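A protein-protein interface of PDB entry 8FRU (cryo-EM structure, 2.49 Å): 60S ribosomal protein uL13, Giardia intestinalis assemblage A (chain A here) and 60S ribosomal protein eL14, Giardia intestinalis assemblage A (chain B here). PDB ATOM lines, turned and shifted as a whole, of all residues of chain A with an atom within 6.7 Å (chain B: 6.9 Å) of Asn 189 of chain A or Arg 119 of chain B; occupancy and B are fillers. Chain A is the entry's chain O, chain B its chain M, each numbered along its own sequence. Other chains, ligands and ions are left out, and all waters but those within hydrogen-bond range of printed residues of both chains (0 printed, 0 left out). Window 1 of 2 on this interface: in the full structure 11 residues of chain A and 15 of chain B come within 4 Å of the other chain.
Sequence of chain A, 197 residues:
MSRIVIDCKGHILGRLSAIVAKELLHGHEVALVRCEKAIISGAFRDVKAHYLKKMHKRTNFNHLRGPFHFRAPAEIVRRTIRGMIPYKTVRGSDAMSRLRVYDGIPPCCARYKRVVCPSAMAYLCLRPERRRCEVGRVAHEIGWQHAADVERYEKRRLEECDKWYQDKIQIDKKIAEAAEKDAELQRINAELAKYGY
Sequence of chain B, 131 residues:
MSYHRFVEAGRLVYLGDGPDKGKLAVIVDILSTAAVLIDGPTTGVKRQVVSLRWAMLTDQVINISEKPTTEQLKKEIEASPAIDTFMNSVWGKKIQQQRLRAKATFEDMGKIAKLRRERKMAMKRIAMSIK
The guanidinium group (NH2) of Arg 119 of chain B is in hydrogen-bond range of the backbone carbonyl oxygen (O) of Tyr 197 of chain A, at 3.2 Å.
N of Tyr 197 of chain A lies within hydrogen-bond range of O of Leu 192 of chain A, 3.3 Å away.
O of Leu 185 of chain A sits close to ND2 of Asn 189 of chain A (3.3 Å).
Among the printed residues, merely in contact across the chains: Leu 185 of chain A with Met 123 of chain B (3.2 Å), Leu 192 of chain A with Arg 119 of chain B (3.5 Å), Ile 188 of chain A with Glu 118 of chain B (3.7 Å), Leu 185 of chain A with Ala 122 of chain B (3.8 Å), Asn 189 of chain A with Arg 119 of chain B (3.8 Å), Ile 188 of chain A with Arg 119 of chain B (3.9 Å) and Leu 192 of chain A with Leu 115 of chain B (3.9 Å).
Gln 186 of chain A touches none of the printed residues of chain B.
Asn 189 of chain A touches just one residue of chain B: Arg 119.
Printed residues of chain B within 4 Å of Tyr 197 of chain A: Arg 119 (3.2 Å).
Of the printed residues of chain A, Leu 115 of chain B touches Leu 192 (3.9 Å).
Printed residues of chain A within 4 Å of Glu 118 of chain B: Ile 188.
Arg 119 of chain B touches four residues of chain A.
Printed residues of chain A within 4 Å of Met 123 of chain B: Leu 185.
The nearest residue of chain B that does not touch Asn 189 of chain A is Met 123 of chain B (6.1 Å).
The nearest residue of chain A that does not touch Arg 119 of chain B is Leu 185 of chain A (4.1 Å).
The nearest printed residue of chain B that does not touch Tyr 197 of chain A is Arg 116 of chain B (4.02 Å).
Along chain B the printed residues that touch a printed residue of chain A span positions 115 to 123.
Of the 13 printed residues of chain A, 5 touch a printed residue of chain B.
Hydrophobic or aromatic side chains of chain A that line the printed part of chain B: Leu 185, Ile 188 and Leu 192.
Among the printed residues, 8 pairs touch across the chains.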
ATOM      1  N   ALA A 179     -22.016 -24.267 -27.680  1.00  0.00           N
ATOM      2  CA  ALA A 179     -20.668 -24.761 -27.425  1.00  0.00           C
ATOM      3  C   ALA A 179     -20.391 -24.860 -25.933  1.00  0.00           C
ATOM      4  O   ALA A 179     -19.760 -25.818 -25.473  1.00  0.00           O
ATOM      5  CB  ALA A 179     -19.638 -23.857 -28.100  1.00  0.00           C
ATOM      6  N   GLU A 184     -18.373 -32.693 -25.063  1.00  0.00           N
ATOM      7  CA  GLU A 184     -17.152 -33.167 -25.702  1.00  0.00           C
ATOM      8  C   GLU A 184     -16.116 -32.054 -25.810  1.00  0.00           C
ATOM      9  O   GLU A 184     -14.922 -32.281 -25.590  1.00  0.00           O
ATOM     10  CB  GLU A 184     -17.477 -33.736 -27.079  1.00  0.00           C
ATOM     11  CG  GLU A 184     -16.506 -34.781 -27.552  1.00  0.00           C
ATOM     12  CD  GLU A 184     -15.289 -34.158 -28.180  1.00  0.00           C
ATOM     13  OE1 GLU A 184     -15.372 -32.973 -28.557  1.00  0.00           O
ATOM     14  OE2 GLU A 184     -14.252 -34.845 -28.295  1.00  0.00           O
ATOM     15  N   LEU A 185     -16.555 -30.844 -26.155  1.00  0.00           N
ATOM     16  CA  LEU A 185     -15.634 -29.722 -26.242  1.00  0.00           C
ATOM     17  C   LEU A 185     -15.016 -29.396 -24.891  1.00  0.00           C
ATOM     18  O   LEU A 185     -13.857 -28.975 -24.825  1.00  0.00           O
ATOM     19  CB  LEU A 185     -16.361 -28.501 -26.800  1.00  0.00           C
ATOM     20  CG  LEU A 185     -15.503 -27.402 -27.418  1.00  0.00           C
ATOM     21  CD1 LEU A 185     -14.548 -27.996 -28.436  1.00  0.00           C
ATOM     22  CD2 LEU A 185     -16.392 -26.347 -28.053  1.00  0.00           C
ATOM     23  N   GLN A 186     -15.764 -29.583 -23.804  1.00  0.00           N
ATOM     24  CA  GLN A 186     -15.231 -29.268 -22.484  1.00  0.00           C
ATOM     25  C   GLN A 186     -13.987 -30.092 -22.187  1.00  0.00           C
ATOM     26  O   GLN A 186     -13.014 -29.584 -21.619  1.00  0.00           O
ATOM     27  CB  GLN A 186     -16.296 -29.513 -21.417  1.00  0.00           C
ATOM     28  CG  GLN A 186     -17.709 -29.309 -21.909  1.00  0.00           C
ATOM     29  CD  GLN A 186     -18.586 -28.579 -20.911  1.00  0.00           C
ATOM     30  OE1 GLN A 186     -18.360 -28.641 -19.704  1.00  0.00           O
ATOM     31  NE2 GLN A 186     -19.595 -27.879 -21.415  1.00  0.00           N
ATOM     32  N   ARG A 187     -14.008 -31.374 -22.552  1.00  0.00           N
ATOM     33  CA  ARG A 187     -12.844 -32.225 -22.341  1.00  0.00           C
ATOM     34  C   ARG A 187     -11.637 -31.703 -23.111  1.00  0.00           C
ATOM     35  O   ARG A 187     -10.528 -31.628 -22.570  1.00  0.00           O
ATOM     36  CB  ARG A 187     -13.177 -33.657 -22.757  1.00  0.00           C
ATOM     37  CG  ARG A 187     -12.155 -34.695 -22.343  1.00  0.00           C
ATOM     38  CD  ARG A 187     -12.262 -35.939 -23.206  1.00  0.00           C
ATOM     39  NE  ARG A 187     -11.614 -35.755 -24.498  1.00  0.00           N
ATOM     40  CZ  ARG A 187     -11.722 -36.589 -25.523  1.00  0.00           C
ATOM     41  NH1 ARG A 187     -12.437 -37.699 -25.442  1.00  0.00           N
ATOM     42  NH2 ARG A 187     -11.097 -36.302 -26.662  1.00  0.00           N
ATOM     43  N   ILE A 188     -11.840 -31.325 -24.374  1.00  0.00           N
ATOM     44  CA  ILE A 188     -10.748 -30.804 -25.189  1.00  0.00           C
ATOM     45  C   ILE A 188     -10.207 -29.512 -24.595  1.00  0.00           C
ATOM     46  O   ILE A 188      -8.989 -29.306 -24.524  1.00  0.00           O
ATOM     47  CB  ILE A 188     -11.222 -30.597 -26.638  1.00  0.00           C
ATOM     48  CG1 ILE A 188     -11.287 -31.932 -27.376  1.00  0.00           C
ATOM     49  CG2 ILE A 188     -10.316 -29.618 -27.366  1.00  0.00           C
ATOM     50  CD1 ILE A 188     -12.049 -31.860 -28.674  1.00  0.00           C
ATOM     51  N   ASN A 189     -11.099 -28.612 -24.181  1.00  0.00           N
ATOM     52  CA  ASN A 189     -10.646 -27.354 -23.601  1.00  0.00           C
ATOM     53  C   ASN A 189      -9.848 -27.591 -22.327  1.00  0.00           C
ATOM     54  O   ASN A 189      -8.808 -26.961 -22.113  1.00  0.00           O
ATOM     55  CB  ASN A 189     -11.836 -26.443 -23.323  1.00  0.00           C
ATOM     56  CG  ASN A 189     -12.633 -26.134 -24.565  1.00  0.00           C
ATOM     57  OD1 ASN A 189     -12.141 -26.266 -25.681  1.00  0.00           O
ATOM     58  ND2 ASN A 189     -13.873 -25.709 -24.378  1.00  0.00           N
ATOM     59  N   ALA A 190     -10.321 -28.494 -21.469  1.00  0.00           N
ATOM     60  CA  ALA A 190      -9.579 -28.799 -20.250  1.00  0.00           C
ATOM     61  C   ALA A 190      -8.214 -29.385 -20.573  1.00  0.00           C
ATOM     62  O   ALA A 190      -7.213 -29.036 -19.938  1.00  0.00           O
ATOM     63  CB  ALA A 190     -10.379 -29.760 -19.373  1.00  0.00           C
ATOM     64  N   GLU A 191      -8.150 -30.279 -21.559  1.00  0.00           N
ATOM     65  CA  GLU A 191      -6.872 -30.868 -21.937  1.00  0.00           C
ATOM     66  C   GLU A 191      -5.906 -29.811 -22.451  1.00  0.00           C
ATOM     67  O   GLU A 191      -4.716 -29.834 -22.120  1.00  0.00           O
ATOM     68  CB  GLU A 191      -7.093 -31.949 -22.990  1.00  0.00           C
ATOM     69  CG  GLU A 191      -7.188 -33.341 -22.425  1.00  0.00           C
ATOM     70  CD  GLU A 191      -5.863 -34.066 -22.447  1.00  0.00           C
ATOM     71  OE1 GLU A 191      -5.472 -34.556 -23.526  1.00  0.00           O
ATOM     72  OE2 GLU A 191      -5.211 -34.146 -21.385  1.00  0.00           O
ATOM     73  N   LEU A 192      -6.398 -28.876 -23.265  1.00  0.00           N
ATOM     74  CA  LEU A 192      -5.534 -27.825 -23.792  1.00  0.00           C
ATOM     75  C   LEU A 192      -5.123 -26.834 -22.714  1.00  0.00           C
ATOM     76  O   LEU A 192      -4.056 -26.222 -22.814  1.00  0.00           O
ATOM     77  CB  LEU A 192      -6.230 -27.090 -24.935  1.00  0.00           C
ATOM     78  CG  LEU A 192      -5.948 -27.571 -26.358  1.00  0.00           C
ATOM     79  CD1 LEU A 192      -6.739 -26.750 -27.351  1.00  0.00           C
ATOM     80  CD2 LEU A 192      -4.461 -27.519 -26.673  1.00  0.00           C
ATOM     81  N   ALA A 193      -5.951 -26.649 -21.686  1.00  0.00           N
ATOM     82  CA  ALA A 193      -5.632 -25.676 -20.650  1.00  0.00           C
ATOM     83  C   ALA A 193      -4.383 -26.050 -19.868  1.00  0.00           C
ATOM     84  O   ALA A 193      -3.753 -25.170 -19.274  1.00  0.00           O
ATOM     85  CB  ALA A 193      -6.811 -25.512 -19.695  1.00  0.00           C
ATOM     86  N   LYS A 194      -4.013 -27.330 -19.852  1.00  0.00           N
ATOM     87  CA  LYS A 194      -2.805 -27.744 -19.150  1.00  0.00           C
ATOM     88  C   LYS A 194      -1.545 -27.237 -19.832  1.00  0.00           C
ATOM     89  O   LYS A 194      -0.501 -27.139 -19.181  1.00  0.00           O
ATOM     90  CB  LYS A 194      -2.759 -29.265 -19.042  1.00  0.00           C
ATOM     91  CG  LYS A 194      -4.087 -29.883 -18.655  1.00  0.00           C
ATOM     92  CD  LYS A 194      -3.923 -30.984 -17.630  1.00  0.00           C
ATOM     93  CE  LYS A 194      -3.811 -30.417 -16.231  1.00  0.00           C
ATOM     94  NZ  LYS A 194      -4.791 -29.322 -15.993  1.00  0.00           N
ATOM     95  N   TYR A 197      -3.181 -23.157 -23.452  1.00  0.00           N
ATOM     96  CA  TYR A 197      -3.842 -22.805 -24.702  1.00  0.00           C
ATOM     97  C   TYR A 197      -5.356 -22.916 -24.588  1.00  0.00           C
ATOM     98  O   TYR A 197      -6.049 -23.091 -25.587  1.00  0.00           O
ATOM     99  CB  TYR A 197      -3.340 -23.693 -25.837  1.00  0.00           C
ATOM    100  CG  TYR A 197      -2.061 -23.200 -26.451  1.00  0.00           C
ATOM    101  CD1 TYR A 197      -2.060 -22.116 -27.311  1.00  0.00           C
ATOM    102  CD2 TYR A 197      -0.851 -23.803 -26.158  1.00  0.00           C
ATOM    103  CE1 TYR A 197      -0.891 -21.653 -27.870  1.00  0.00           C
ATOM    104  CE2 TYR A 197       0.319 -23.344 -26.712  1.00  0.00           C
ATOM    105  CZ  TYR A 197       0.291 -22.268 -27.567  1.00  0.00           C
ATOM    106  OH  TYR A 197       1.456 -21.803 -28.125  1.00  0.00           O
ATOM    107  N   LYS B 114      -2.544 -31.967 -32.260  1.00  0.00           N
ATOM    108  CA  LYS B 114      -3.613 -32.952 -32.361  1.00  0.00           C
ATOM    109  C   LYS B 114      -4.877 -32.470 -31.663  1.00  0.00           C
ATOM    110  O   LYS B 114      -5.983 -32.633 -32.188  1.00  0.00           O
ATOM    111  CB  LYS B 114      -3.148 -34.284 -31.777  1.00  0.00           C
ATOM    112  CG  LYS B 114      -4.197 -35.368 -31.805  1.00  0.00           C
ATOM    113  CD  LYS B 114      -4.103 -36.195 -33.064  1.00  0.00           C
ATOM    114  CE  LYS B 114      -5.468 -36.717 -33.464  1.00  0.00           C
ATOM    115  NZ  LYS B 114      -6.146 -35.817 -34.438  1.00  0.00           N
ATOM    116  N   LEU B 115      -4.733 -31.883 -30.474  1.00  0.00           N
ATOM    117  CA  LEU B 115      -5.889 -31.347 -29.762  1.00  0.00           C
ATOM    118  C   LEU B 115      -6.502 -30.166 -30.501  1.00  0.00           C
ATOM    119  O   LEU B 115      -7.726 -30.002 -30.515  1.00  0.00           O
ATOM    120  CB  LEU B 115      -5.488 -30.943 -28.348  1.00  0.00           C
ATOM    121  CG  LEU B 115      -5.316 -32.112 -27.381  1.00  0.00           C
ATOM    122  CD1 LEU B 115      -4.532 -31.690 -26.160  1.00  0.00           C
ATOM    123  CD2 LEU B 115      -6.666 -32.668 -26.993  1.00  0.00           C
ATOM    124  N   ARG B 116      -5.666 -29.317 -31.104  1.00  0.00           N
ATOM    125  CA  ARG B 116      -6.190 -28.205 -31.889  1.00  0.00           C
ATOM    126  C   ARG B 116      -7.027 -28.703 -33.055  1.00  0.00           C
ATOM    127  O   ARG B 116      -8.067 -28.120 -33.376  1.00  0.00           O
ATOM    128  CB  ARG B 116      -5.047 -27.332 -32.398  1.00  0.00           C
ATOM    129  CG  ARG B 116      -4.601 -26.257 -31.440  1.00  0.00           C
ATOM    130  CD  ARG B 116      -4.068 -25.061 -32.199  1.00  0.00           C
ATOM    131  NE  ARG B 116      -2.944 -24.436 -31.515  1.00  0.00           N
ATOM    132  CZ  ARG B 116      -1.671 -24.695 -31.775  1.00  0.00           C
ATOM    133  NH1 ARG B 116      -1.319 -25.557 -32.713  1.00  0.00           N
ATOM    134  NH2 ARG B 116      -0.729 -24.067 -31.081  1.00  0.00           N
ATOM    135  N   ARG B 117      -6.582 -29.775 -33.709  1.00  0.00           N
ATOM    136  CA  ARG B 117      -7.338 -30.336 -34.822  1.00  0.00           C
ATOM    137  C   ARG B 117      -8.714 -30.802 -34.364  1.00  0.00           C
ATOM    138  O   ARG B 117      -9.721 -30.553 -35.031  1.00  0.00           O
ATOM    139  CB  ARG B 117      -6.552 -31.484 -35.457  1.00  0.00           C
ATOM    140  CG  ARG B 117      -7.236 -32.139 -36.641  1.00  0.00           C
ATOM    141  CD  ARG B 117      -7.667 -31.115 -37.665  1.00  0.00           C
ATOM    142  NE  ARG B 117      -8.400 -31.720 -38.765  1.00  0.00           N
ATOM    143  CZ  ARG B 117      -8.336 -31.313 -40.025  1.00  0.00           C
ATOM    144  NH1 ARG B 117      -7.567 -30.298 -40.385  1.00  0.00           N
ATOM    145  NH2 ARG B 117      -9.065 -31.933 -40.944  1.00  0.00           N
ATOM    146  N   GLU B 118      -8.775 -31.470 -33.214  1.00  0.00           N
ATOM    147  CA  GLU B 118     -10.060 -31.921 -32.691  1.00  0.00           C
ATOM    148  C   GLU B 118     -10.974 -30.744 -32.378  1.00  0.00           C
ATOM    149  O   GLU B 118     -12.180 -30.800 -32.637  1.00  0.00           O
ATOM    150  CB  GLU B 118      -9.844 -32.782 -31.448  1.00  0.00           C
ATOM    151  CG  GLU B 118      -8.767 -33.832 -31.614  1.00  0.00           C
ATOM    152  CD  GLU B 118      -8.243 -34.345 -30.290  1.00  0.00           C
ATOM    153  OE1 GLU B 118      -8.174 -33.554 -29.326  1.00  0.00           O
ATOM    154  OE2 GLU B 118      -7.891 -35.542 -30.212  1.00  0.00           O
ATOM    155  N   ARG B 119     -10.422 -29.672 -31.814  1.00  0.00           N
ATOM    156  CA  ARG B 119     -11.240 -28.514 -31.474  1.00  0.00           C
ATOM    157  C   ARG B 119     -11.824 -27.862 -32.720  1.00  0.00           C
ATOM    158  O   ARG B 119     -12.986 -27.445 -32.724  1.00  0.00           O
ATOM    159  CB  ARG B 119     -10.411 -27.512 -30.677  1.00  0.00           C
ATOM    160  CG  ARG B 119     -11.193 -26.338 -30.151  1.00  0.00           C
ATOM    161  CD  ARG B 119     -10.305 -25.132 -29.973  1.00  0.00           C
ATOM    162  NE  ARG B 119     -10.028 -24.871 -28.566  1.00  0.00           N
ATOM    163  CZ  ARG B 119      -9.021 -24.132 -28.124  1.00  0.00           C
ATOM    164  NH1 ARG B 119      -8.182 -23.538 -28.955  1.00  0.00           N
ATOM    165  NH2 ARG B 119      -8.852 -23.986 -26.815  1.00  0.00           N
ATOM    166  N   LYS B 120     -11.030 -27.755 -33.785  1.00  0.00           N
ATOM    167  CA  LYS B 120     -11.543 -27.192 -35.029  1.00  0.00           C
ATOM    168  C   LYS B 120     -12.654 -28.053 -35.605  1.00  0.00           C
ATOM    169  O   LYS B 120     -13.640 -27.536 -36.138  1.00  0.00           O
ATOM    170  CB  LYS B 120     -10.417 -27.042 -36.046  1.00  0.00           C
ATOM    171  CG  LYS B 120     -10.848 -26.354 -37.314  1.00  0.00           C
ATOM    172  CD  LYS B 120      -9.668 -26.008 -38.178  1.00  0.00           C
ATOM    173  CE  LYS B 120      -9.348 -27.120 -39.144  1.00  0.00           C
ATOM    174  NZ  LYS B 120      -8.883 -26.574 -40.447  1.00  0.00           N
ATOM    175  N   MET B 121     -12.493 -29.371 -35.548  1.00  0.00           N
ATOM    176  CA  MET B 121     -13.537 -30.262 -36.033  1.00  0.00           C
ATOM    177  C   MET B 121     -14.771 -30.203 -35.144  1.00  0.00           C
ATOM    178  O   MET B 121     -15.903 -30.232 -35.637  1.00  0.00           O
ATOM    179  CB  MET B 121     -12.994 -31.684 -36.127  1.00  0.00           C
ATOM    180  CG  MET B 121     -11.898 -31.820 -37.160  1.00  0.00           C
ATOM    181  SD  MET B 121     -12.499 -31.480 -38.822  1.00  0.00           S
ATOM    182  CE  MET B 121     -11.724 -29.906 -39.160  1.00  0.00           C
ATOM    183  N   ALA B 122     -14.575 -30.129 -33.828  1.00  0.00           N
ATOM    184  CA  ALA B 122     -15.714 -30.036 -32.923  1.00  0.00           C
ATOM    185  C   ALA B 122     -16.483 -28.740 -33.138  1.00  0.00           C
ATOM    186  O   ALA B 122     -17.716 -28.725 -33.074  1.00  0.00           O
ATOM    187  CB  ALA B 122     -15.246 -30.154 -31.475  1.00  0.00           C
ATOM    188  N   MET B 123     -15.773 -27.639 -33.387  1.00  0.00           N
ATOM    189  CA  MET B 123     -16.447 -26.369 -33.632  1.00  0.00           C
ATOM    190  C   MET B 123     -17.308 -26.431 -34.885  1.00  0.00           C
ATOM    191  O   MET B 123     -18.432 -25.917 -34.903  1.00  0.00           O
ATOM    192  CB  MET B 123     -15.422 -25.244 -33.754  1.00  0.00           C
ATOM    193  CG  MET B 123     -15.786 -23.983 -33.001  1.00  0.00           C
ATOM    194  SD  MET B 123     -16.211 -24.288 -31.281  1.00  0.00           S
ATOM    195  CE  MET B 123     -15.208 -25.726 -30.935  1.00  0.00           C
ATOM    196  N   LYS B 124     -16.792 -27.041 -35.950  1.00  0.00           N
ATOM    197  CA  LYS B 124     -17.547 -27.121 -37.195  1.00  0.00           C
ATOM    198  C   LYS B 124     -18.832 -27.917 -37.007  1.00  0.00           C
ATOM    199  O   LYS B 124     -19.899 -27.524 -37.489  1.00  0.00           O
ATOM    200  CB  LYS B 124     -16.678 -27.743 -38.286  1.00  0.00           C
ATOM    201  CG  LYS B 124     -17.255 -27.655 -39.678  1.00  0.00           C
ATOM    202  CD  LYS B 124     -16.912 -28.904 -40.466  1.00  0.00           C
ATOM    203  CE  LYS B 124     -16.824 -28.622 -41.956  1.00  0.00           C
ATOM    204  NZ  LYS B 124     -16.071 -29.694 -42.659  1.00  0.00           N
